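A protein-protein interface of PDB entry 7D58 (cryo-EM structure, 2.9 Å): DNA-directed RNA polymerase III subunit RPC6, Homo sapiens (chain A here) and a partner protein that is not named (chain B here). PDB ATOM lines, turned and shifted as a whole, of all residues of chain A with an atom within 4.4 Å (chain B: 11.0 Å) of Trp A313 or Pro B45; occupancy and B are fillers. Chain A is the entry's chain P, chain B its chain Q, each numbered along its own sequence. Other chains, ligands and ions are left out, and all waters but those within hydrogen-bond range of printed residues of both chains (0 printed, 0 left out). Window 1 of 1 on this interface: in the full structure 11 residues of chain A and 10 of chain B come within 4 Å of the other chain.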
ATOM      1  N   ARG A 284     -27.220  15.164  20.744  1.00  0.00           N
ATOM      2  CA  ARG A 284     -27.692  13.931  21.368  1.00  0.00           C
ATOM      3  C   ARG A 284     -26.794  12.748  21.027  1.00  0.00           C
ATOM      4  O   ARG A 284     -26.759  11.763  21.774  1.00  0.00           O
ATOM      5  CB  ARG A 284     -29.134  13.650  20.950  1.00  0.00           C
ATOM      6  CG  ARG A 284     -30.121  14.689  21.455  1.00  0.00           C
ATOM      7  CD  ARG A 284     -31.471  14.566  20.775  1.00  0.00           C
ATOM      8  NE  ARG A 284     -32.413  15.558  21.282  1.00  0.00           N
ATOM      9  CZ  ARG A 284     -33.576  15.847  20.708  1.00  0.00           C
ATOM     10  NH1 ARG A 284     -33.947  15.215  19.605  1.00  0.00           N
ATOM     11  NH2 ARG A 284     -34.368  16.768  21.240  1.00  0.00           N
ATOM     12  N   PRO A 286     -23.099  11.079  20.917  1.00  0.00           N
ATOM     13  CA  PRO A 286     -21.913  11.312  21.756  1.00  0.00           C
ATOM     14  C   PRO A 286     -20.752  11.963  21.025  1.00  0.00           C
ATOM     15  O   PRO A 286     -19.811  12.421  21.688  1.00  0.00           O
ATOM     16  CB  PRO A 286     -21.540   9.902  22.238  1.00  0.00           C
ATOM     17  CG  PRO A 286     -22.120   8.988  21.218  1.00  0.00           C
ATOM     18  CD  PRO A 286     -23.375   9.646  20.725  1.00  0.00           C
ATOM     19  N   LEU A 289     -20.283  15.649  22.171  1.00  0.00           N
ATOM     20  CA  LEU A 289     -19.656  15.845  23.471  1.00  0.00           C
ATOM     21  C   LEU A 289     -18.192  15.429  23.492  1.00  0.00           C
ATOM     22  O   LEU A 289     -17.499  15.711  24.476  1.00  0.00           O
ATOM     23  CB  LEU A 289     -20.402  15.059  24.558  1.00  0.00           C
ATOM     24  CG  LEU A 289     -21.669  15.637  25.196  1.00  0.00           C
ATOM     25  CD1 LEU A 289     -21.395  16.985  25.855  1.00  0.00           C
ATOM     26  CD2 LEU A 289     -22.809  15.724  24.200  1.00  0.00           C
ATOM     27  N   TYR A 309     -16.773   6.238  24.621  1.00  0.00           N
ATOM     28  CA  TYR A 309     -18.031   6.977  24.685  1.00  0.00           C
ATOM     29  C   TYR A 309     -19.121   6.281  23.878  1.00  0.00           C
ATOM     30  O   TYR A 309     -20.274   6.199  24.317  1.00  0.00           O
ATOM     31  CB  TYR A 309     -17.826   8.407  24.190  1.00  0.00           C
ATOM     32  CG  TYR A 309     -16.675   9.127  24.850  1.00  0.00           C
ATOM     33  CD1 TYR A 309     -16.786   9.610  26.147  1.00  0.00           C
ATOM     34  CD2 TYR A 309     -15.478   9.327  24.175  1.00  0.00           C
ATOM     35  CE1 TYR A 309     -15.735  10.269  26.755  1.00  0.00           C
ATOM     36  CE2 TYR A 309     -14.423   9.984  24.774  1.00  0.00           C
ATOM     37  CZ  TYR A 309     -14.557  10.452  26.062  1.00  0.00           C
ATOM     38  OH  TYR A 309     -13.505  11.107  26.656  1.00  0.00           O
ATOM     39  N   MET A 310     -18.775   5.777  22.691  1.00  0.00           N
ATOM     40  CA  MET A 310     -19.749   5.077  21.861  1.00  0.00           C
ATOM     41  C   MET A 310     -20.285   3.840  22.574  1.00  0.00           C
ATOM     42  O   MET A 310     -21.494   3.581  22.580  1.00  0.00           O
ATOM     43  CB  MET A 310     -19.117   4.697  20.520  1.00  0.00           C
ATOM     44  CG  MET A 310     -18.786   5.880  19.622  1.00  0.00           C
ATOM     45  SD  MET A 310     -20.232   6.852  19.161  1.00  0.00           S
ATOM     46  CE  MET A 310     -21.144   5.670  18.176  1.00  0.00           C
ATOM     47  N   THR A 311     -19.390   3.065  23.190  1.00  0.00           N
ATOM     48  CA  THR A 311     -19.808   1.863  23.903  1.00  0.00           C
ATOM     49  C   THR A 311     -20.669   2.212  25.112  1.00  0.00           C
ATOM     50  O   THR A 311     -21.678   1.551  25.386  1.00  0.00           O
ATOM     51  CB  THR A 311     -18.580   1.054  24.328  1.00  0.00           C
ATOM     52  OG1 THR A 311     -17.889   0.585  23.163  1.00  0.00           O
ATOM     53  CG2 THR A 311     -18.990  -0.140  25.177  1.00  0.00           C
ATOM     54  N   GLU A 312     -20.283   3.256  25.849  1.00  0.00           N
ATOM     55  CA  GLU A 312     -21.045   3.652  27.030  1.00  0.00           C
ATOM     56  C   GLU A 312     -22.416   4.193  26.643  1.00  0.00           C
ATOM     57  O   GLU A 312     -23.377   4.098  27.415  1.00  0.00           O
ATOM     58  CB  GLU A 312     -20.260   4.687  27.837  1.00  0.00           C
ATOM     59  CG  GLU A 312     -19.199   4.082  28.743  1.00  0.00           C
ATOM     60  CD  GLU A 312     -18.795   5.010  29.872  1.00  0.00           C
ATOM     61  OE1 GLU A 312     -19.082   6.222  29.780  1.00  0.00           O
ATOM     62  OE2 GLU A 312     -18.187   4.527  30.851  1.00  0.00           O
ATOM     63  N   TRP A 313     -22.525   4.774  25.446  1.00  0.00           N
ATOM     64  CA  TRP A 313     -23.825   5.221  24.957  1.00  0.00           C
ATOM     65  C   TRP A 313     -24.672   4.040  24.497  1.00  0.00           C
ATOM     66  O   TRP A 313     -25.892   4.019  24.695  1.00  0.00           O
ATOM     67  CB  TRP A 313     -23.638   6.226  23.820  1.00  0.00           C
ATOM     68  CG  TRP A 313     -24.911   6.889  23.395  1.00  0.00           C
ATOM     69  CD1 TRP A 313     -25.760   7.613  24.181  1.00  0.00           C
ATOM     70  CD2 TRP A 313     -25.486   6.882  22.083  1.00  0.00           C
ATOM     71  NE1 TRP A 313     -26.826   8.061  23.439  1.00  0.00           N
ATOM     72  CE2 TRP A 313     -26.682   7.626  22.148  1.00  0.00           C
ATOM     73  CE3 TRP A 313     -25.106   6.322  20.860  1.00  0.00           C
ATOM     74  CZ2 TRP A 313     -27.499   7.822  21.036  1.00  0.00           C
ATOM     75  CZ3 TRP A 313     -25.918   6.519  19.759  1.00  0.00           C
ATOM     76  CH2 TRP A 313     -27.101   7.263  19.854  1.00  0.00           C
ATOM     77  N   LEU A 314     -24.035   3.047  23.875  1.00  0.00           N
ATOM     78  CA  LEU A 314     -24.774   1.898  23.360  1.00  0.00           C
ATOM     79  C   LEU A 314     -25.293   1.019  24.493  1.00  0.00           C
ATOM     80  O   LEU A 314     -26.405   0.484  24.417  1.00  0.00           O
ATOM     81  CB  LEU A 314     -23.890   1.087  22.411  1.00  0.00           C
ATOM     82  CG  LEU A 314     -23.631   1.694  21.031  1.00  0.00           C
ATOM     83  CD1 LEU A 314     -22.783   0.759  20.182  1.00  0.00           C
ATOM     84  CD2 LEU A 314     -24.940   2.024  20.330  1.00  0.00           C
ATOM     85  N   GLU A 315     -24.496   0.852  25.551  1.00  0.00           N
ATOM     86  CA  GLU A 315     -24.891  -0.028  26.648  1.00  0.00           C
ATOM     87  C   GLU A 315     -26.100   0.528  27.396  1.00  0.00           C
ATOM     88  O   GLU A 315     -26.930  -0.228  27.913  1.00  0.00           O
ATOM     89  CB  GLU A 315     -23.711  -0.247  27.600  1.00  0.00           C
ATOM     90  CG  GLU A 315     -23.172   1.015  28.256  1.00  0.00           C
ATOM     91  CD  GLU A 315     -23.809   1.298  29.603  1.00  0.00           C
ATOM     92  OE1 GLU A 315     -24.298   0.344  30.244  1.00  0.00           O
ATOM     93  OE2 GLU A 315     -23.820   2.475  30.020  1.00  0.00           O
ATOM     94  N   PHE A 316     -26.213   1.850  27.463  1.00  0.00           N
ATOM     95  CA  PHE A 316     -27.325   2.484  28.161  1.00  0.00           C
ATOM     96  C   PHE A 316     -28.561   2.545  27.272  1.00  0.00           C
ATOM     97  O   PHE A 316     -29.553   1.861  27.523  1.00  0.00           O
ATOM     98  CB  PHE A 316     -26.938   3.889  28.630  1.00  0.00           C
ATOM     99  CG  PHE A 316     -27.957   4.531  29.527  1.00  0.00           C
ATOM    100  CD1 PHE A 316     -27.962   4.274  30.889  1.00  0.00           C
ATOM    101  CD2 PHE A 316     -28.909   5.396  29.012  1.00  0.00           C
ATOM    102  CE1 PHE A 316     -28.896   4.863  31.719  1.00  0.00           C
ATOM    103  CE2 PHE A 316     -29.847   5.989  29.838  1.00  0.00           C
ATOM    104  CZ  PHE A 316     -29.840   5.721  31.193  1.00  0.00           C
ATOM    105  N   PHE B  38      -8.672   8.556  26.421  1.00  0.00           N
ATOM    106  CA  PHE B  38     -10.070   8.955  26.568  1.00  0.00           C
ATOM    107  C   PHE B  38     -10.237   9.740  27.861  1.00  0.00           C
ATOM    108  O   PHE B  38     -10.526   9.156  28.915  1.00  0.00           O
ATOM    109  CB  PHE B  38     -11.003   7.741  26.556  1.00  0.00           C
ATOM    110  CG  PHE B  38     -11.108   7.067  25.223  1.00  0.00           C
ATOM    111  CD1 PHE B  38     -12.031   7.501  24.285  1.00  0.00           C
ATOM    112  CD2 PHE B  38     -10.308   5.984  24.916  1.00  0.00           C
ATOM    113  CE1 PHE B  38     -12.135   6.878  23.058  1.00  0.00           C
ATOM    114  CE2 PHE B  38     -10.407   5.355  23.692  1.00  0.00           C
ATOM    115  CZ  PHE B  38     -11.323   5.801  22.762  1.00  0.00           C
ATOM    116  N   ASP B  40     -12.345  11.495  30.428  1.00  0.00           N
ATOM    117  CA  ASP B  40     -13.765  11.443  30.750  1.00  0.00           C
ATOM    118  C   ASP B  40     -14.419  12.811  30.578  1.00  0.00           C
ATOM    119  O   ASP B  40     -13.968  13.807  31.154  1.00  0.00           O
ATOM    120  CB  ASP B  40     -13.943  10.916  32.173  1.00  0.00           C
ATOM    121  CG  ASP B  40     -13.048  11.626  33.173  1.00  0.00           C
ATOM    122  OD1 ASP B  40     -12.224  12.464  32.752  1.00  0.00           O
ATOM    123  OD2 ASP B  40     -13.157  11.337  34.383  1.00  0.00           O
ATOM    124  N   THR B  41     -15.490  12.851  29.788  1.00  0.00           N
ATOM    125  CA  THR B  41     -16.103  14.092  29.339  1.00  0.00           C
ATOM    126  C   THR B  41     -16.695  14.877  30.504  1.00  0.00           C
ATOM    127  O   THR B  41     -16.711  14.431  31.654  1.00  0.00           O
ATOM    128  CB  THR B  41     -17.197  13.816  28.305  1.00  0.00           C
ATOM    129  OG1 THR B  41     -17.776  15.054  27.875  1.00  0.00           O
ATOM    130  CG2 THR B  41     -18.282  12.952  28.909  1.00  0.00           C
ATOM    131  N   ASP B  42     -17.191  16.072  30.182  1.00  0.00           N
ATOM    132  CA  ASP B  42     -17.786  16.943  31.194  1.00  0.00           C
ATOM    133  C   ASP B  42     -19.186  16.465  31.570  1.00  0.00           C
ATOM    134  O   ASP B  42     -19.449  16.124  32.726  1.00  0.00           O
ATOM    135  CB  ASP B  42     -17.816  18.387  30.683  1.00  0.00           C
ATOM    136  CG  ASP B  42     -17.641  19.400  31.793  1.00  0.00           C
ATOM    137  OD1 ASP B  42     -17.252  20.550  31.495  1.00  0.00           O
ATOM    138  OD2 ASP B  42     -17.889  19.046  32.964  1.00  0.00           O
ATOM    139  N   TYR B  43     -20.097  16.436  30.603  1.00  0.00           N
ATOM    140  CA  TYR B  43     -21.454  15.973  30.846  1.00  0.00           C
ATOM    141  C   TYR B  43     -21.796  14.797  29.932  1.00  0.00           C
ATOM    142  O   TYR B  43     -21.068  14.469  28.992  1.00  0.00           O
ATOM    143  CB  TYR B  43     -22.454  17.113  30.652  1.00  0.00           C
ATOM    144  CG  TYR B  43     -21.960  18.460  31.138  1.00  0.00           C
ATOM    145  CD1 TYR B  43     -21.969  18.780  32.490  1.00  0.00           C
ATOM    146  CD2 TYR B  43     -21.496  19.414  30.242  1.00  0.00           C
ATOM    147  CE1 TYR B  43     -21.522  20.012  32.936  1.00  0.00           C
ATOM    148  CE2 TYR B  43     -21.050  20.646  30.679  1.00  0.00           C
ATOM    149  CZ  TYR B  43     -21.064  20.941  32.026  1.00  0.00           C
ATOM    150  OH  TYR B  43     -20.619  22.169  32.462  1.00  0.00           O
ATOM    151  N   LYS B  44     -22.933  14.162  30.216  1.00  0.00           N
ATOM    152  CA  LYS B  44     -23.371  12.996  29.459  1.00  0.00           C
ATOM    153  C   LYS B  44     -24.262  13.429  28.299  1.00  0.00           C
ATOM    154  O   LYS B  44     -24.868  14.507  28.353  1.00  0.00           O
ATOM    155  CB  LYS B  44     -24.109  12.012  30.370  1.00  0.00           C
ATOM    156  CG  LYS B  44     -23.269  11.471  31.516  1.00  0.00           C
ATOM    157  CD  LYS B  44     -22.048  10.726  31.005  1.00  0.00           C
ATOM    158  CE  LYS B  44     -22.448   9.472  30.248  1.00  0.00           C
ATOM    159  NZ  LYS B  44     -23.135   8.488  31.129  1.00  0.00           N
ATOM    160  N   PRO B  45     -24.361  12.632  27.237  1.00  0.00           N
ATOM    161  CA  PRO B  45     -25.194  13.018  26.094  1.00  0.00           C
ATOM    162  C   PRO B  45     -26.677  13.052  26.443  1.00  0.00           C
ATOM    163  O   PRO B  45     -27.116  12.590  27.497  1.00  0.00           O
ATOM    164  CB  PRO B  45     -24.901  11.931  25.053  1.00  0.00           C
ATOM    165  CG  PRO B  45     -24.370  10.780  25.839  1.00  0.00           C
ATOM    166  CD  PRO B  45     -23.619  11.387  26.979  1.00  0.00           C
ATOM    167  N   VAL B  46     -27.447  13.613  25.516  1.00  0.00           N
ATOM    168  CA  VAL B  46     -28.874  13.864  25.705  1.00  0.00           C
ATOM    169  C   VAL B  46     -29.683  12.697  25.150  1.00  0.00           C
ATOM    170  O   VAL B  46     -29.348  12.166  24.080  1.00  0.00           O
ATOM    171  CB  VAL B  46     -29.287  15.185  25.033  1.00  0.00           C
ATOM    172  CG1 VAL B  46     -30.723  15.551  25.383  1.00  0.00           C
ATOM    173  CG2 VAL B  46     -28.329  16.300  25.423  1.00  0.00           C
ATOM    174  N   PRO B  47     -30.737  12.257  25.834  1.00  0.00           N
ATOM    175  CA  PRO B  47     -31.631  11.257  25.244  1.00  0.00           C
ATOM    176  C   PRO B  47     -32.435  11.835  24.090  1.00  0.00           C
ATOM    177  O   PRO B  47     -32.625  13.048  23.970  1.00  0.00           O
ATOM    178  CB  PRO B  47     -32.542  10.860  26.412  1.00  0.00           C
ATOM    179  CG  PRO B  47     -32.485  12.016  27.349  1.00  0.00           C
ATOM    180  CD  PRO B  47     -31.097  12.568  27.227  1.00  0.00           C
ATOM    181  N   LEU B  48     -32.907  10.936  23.231  1.00  0.00           N
ATOM    182  CA  LEU B  48     -33.546  11.321  21.983  1.00  0.00           C
ATOM    183  C   LEU B  48     -35.055  11.474  22.156  1.00  0.00           C
ATOM    184  O   LEU B  48     -35.643  11.068  23.163  1.00  0.00           O
ATOM    185  CB  LEU B  48     -33.249  10.292  20.892  1.00  0.00           C
ATOM    186  CG  LEU B  48     -31.952  10.448  20.094  1.00  0.00           C
ATOM    187  CD1 LEU B  48     -30.729  10.114  20.936  1.00  0.00           C
ATOM    188  CD2 LEU B  48     -32.005   9.577  18.851  1.00  0.00           C
ATOM    189  N   LYS B  49     -35.683  12.070  21.148  1.00  0.00           N
ATOM    190  CA  LYS B  49     -37.131  12.178  21.091  1.00  0.00           C
ATOM    191  C   LYS B  49     -37.713  10.987  20.338  1.00  0.00           C
ATOM    192  O   LYS B  49     -37.167  10.528  19.331  1.00  0.00           O
ATOM    193  CB  LYS B  49     -37.551  13.486  20.414  1.00  0.00           C
ATOM    194  CG  LYS B  49     -37.061  14.750  21.112  1.00  0.00           C
ATOM    195  CD  LYS B  49     -37.735  14.949  22.465  1.00  0.00           C
ATOM    196  CE  LYS B  49     -37.254  16.223  23.149  1.00  0.00           C
ATOM    197  NZ  LYS B  49     -37.725  17.444  22.436  1.00  0.00           N
ATOM    198  N   THR B  50     -38.844  10.490  20.837  1.00  0.00           N
ATOM    199  CA  THR B  50     -39.463   9.284  20.304  1.00  0.00           C
ATOM    200  C   THR B  50     -40.957   9.502  20.125  1.00  0.00           C
ATOM    201  O   THR B  50     -41.640   9.953  21.050  1.00  0.00           O
ATOM    202  CB  THR B  50     -39.218   8.083  21.228  1.00  0.00           C
ATOM    203  OG1 THR B  50     -37.809   7.853  21.353  1.00  0.00           O
ATOM    204  CG2 THR B  50     -39.887   6.830  20.677  1.00  0.00           C
ATOM    205  N   LEU B  58     -37.814   4.833  11.220  1.00  0.00           N
ATOM    206  CA  LEU B  58     -36.717   3.893  11.440  1.00  0.00           C
ATOM    207  C   LEU B  58     -36.910   2.608  10.646  1.00  0.00           C
ATOM    208  O   LEU B  58     -36.003   2.187   9.916  1.00  0.00           O
ATOM    209  CB  LEU B  58     -36.589   3.583  12.930  1.00  0.00           C
ATOM    210  CG  LEU B  58     -35.738   4.561  13.741  1.00  0.00           C
ATOM    211  CD1 LEU B  58     -35.783   4.221  15.221  1.00  0.00           C
ATOM    212  CD2 LEU B  58     -34.309   4.560  13.230  1.00  0.00           C
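OG1 of Thr B41 lies within hydrogen-bond range of O of Leu A289, at 3.5 Å. The backbone carbonyl oxygen (O) of Arg A284 lies close to the backbone carbonyl oxygen (O) of Val B46.
Of the 13 printed residues of chain B, 8 touch a printed residue of chain A. Of the 11 printed residues of chain A, 4 touch a printed residue of chain B. Printed residues of chain A that touch a printed residue of chain B: Arg A284, Leu A289, Tyr A309 and Trp A313. Hydrophobic or aromatic side chains of chain A that line the printed part of chain B: Tyr A309 and Trp A313. Among the printed residues, no Asp or Glu carboxylate lies within 4 Å of a Lys or Arg side-chain nitrogen of the other chain.
Among the printed residues, merely in contact across the chains: Arg A284 with Pro B45, Arg A284 with Pro B47, Arg A284 with Leu B48, Arg A284 with Lys B49, Tyr A309 with Phe B38, Tyr A309 with Asp B40, Tyr A309 with Thr B41, Trp A313 with Pro B45 and Trp A313 with Leu B48.
No residue of chain B comes within 4 Å of Pro A286. Of the printed residues of chain B, Leu A289 touches Thr B41 (3.5 Å). No residue of chain B comes within 4 Å of Met A310. No residue of chain B comes within 4 Å of Glu A312. Trp A313 touches just these residues of chain B: Pro B45 and Leu B48. No residue of chain B comes within 4 Å of Leu A314. No residue of chain B comes within 4 Å of Glu A315. Printed residues of chain A within 4 Å of Asp B40: Tyr A309 (3.97 Å). Of chain A, only Arg A284 (3.8 Å) and Trp A313 (3.8 Å) come within 4 Å of Pro B45. Of the printed residues of chain A, Pro B47 touches Arg A284. Printed residues of chain A within 4 Å of Leu B48: Arg A284 and Trp A313. Of the printed residues of chain A, Lys B49 touches Arg A284 (3.4 Å). The nearest printed residue of chain A that does not touch Pro B47 is Trp A313 (6.0 Å).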
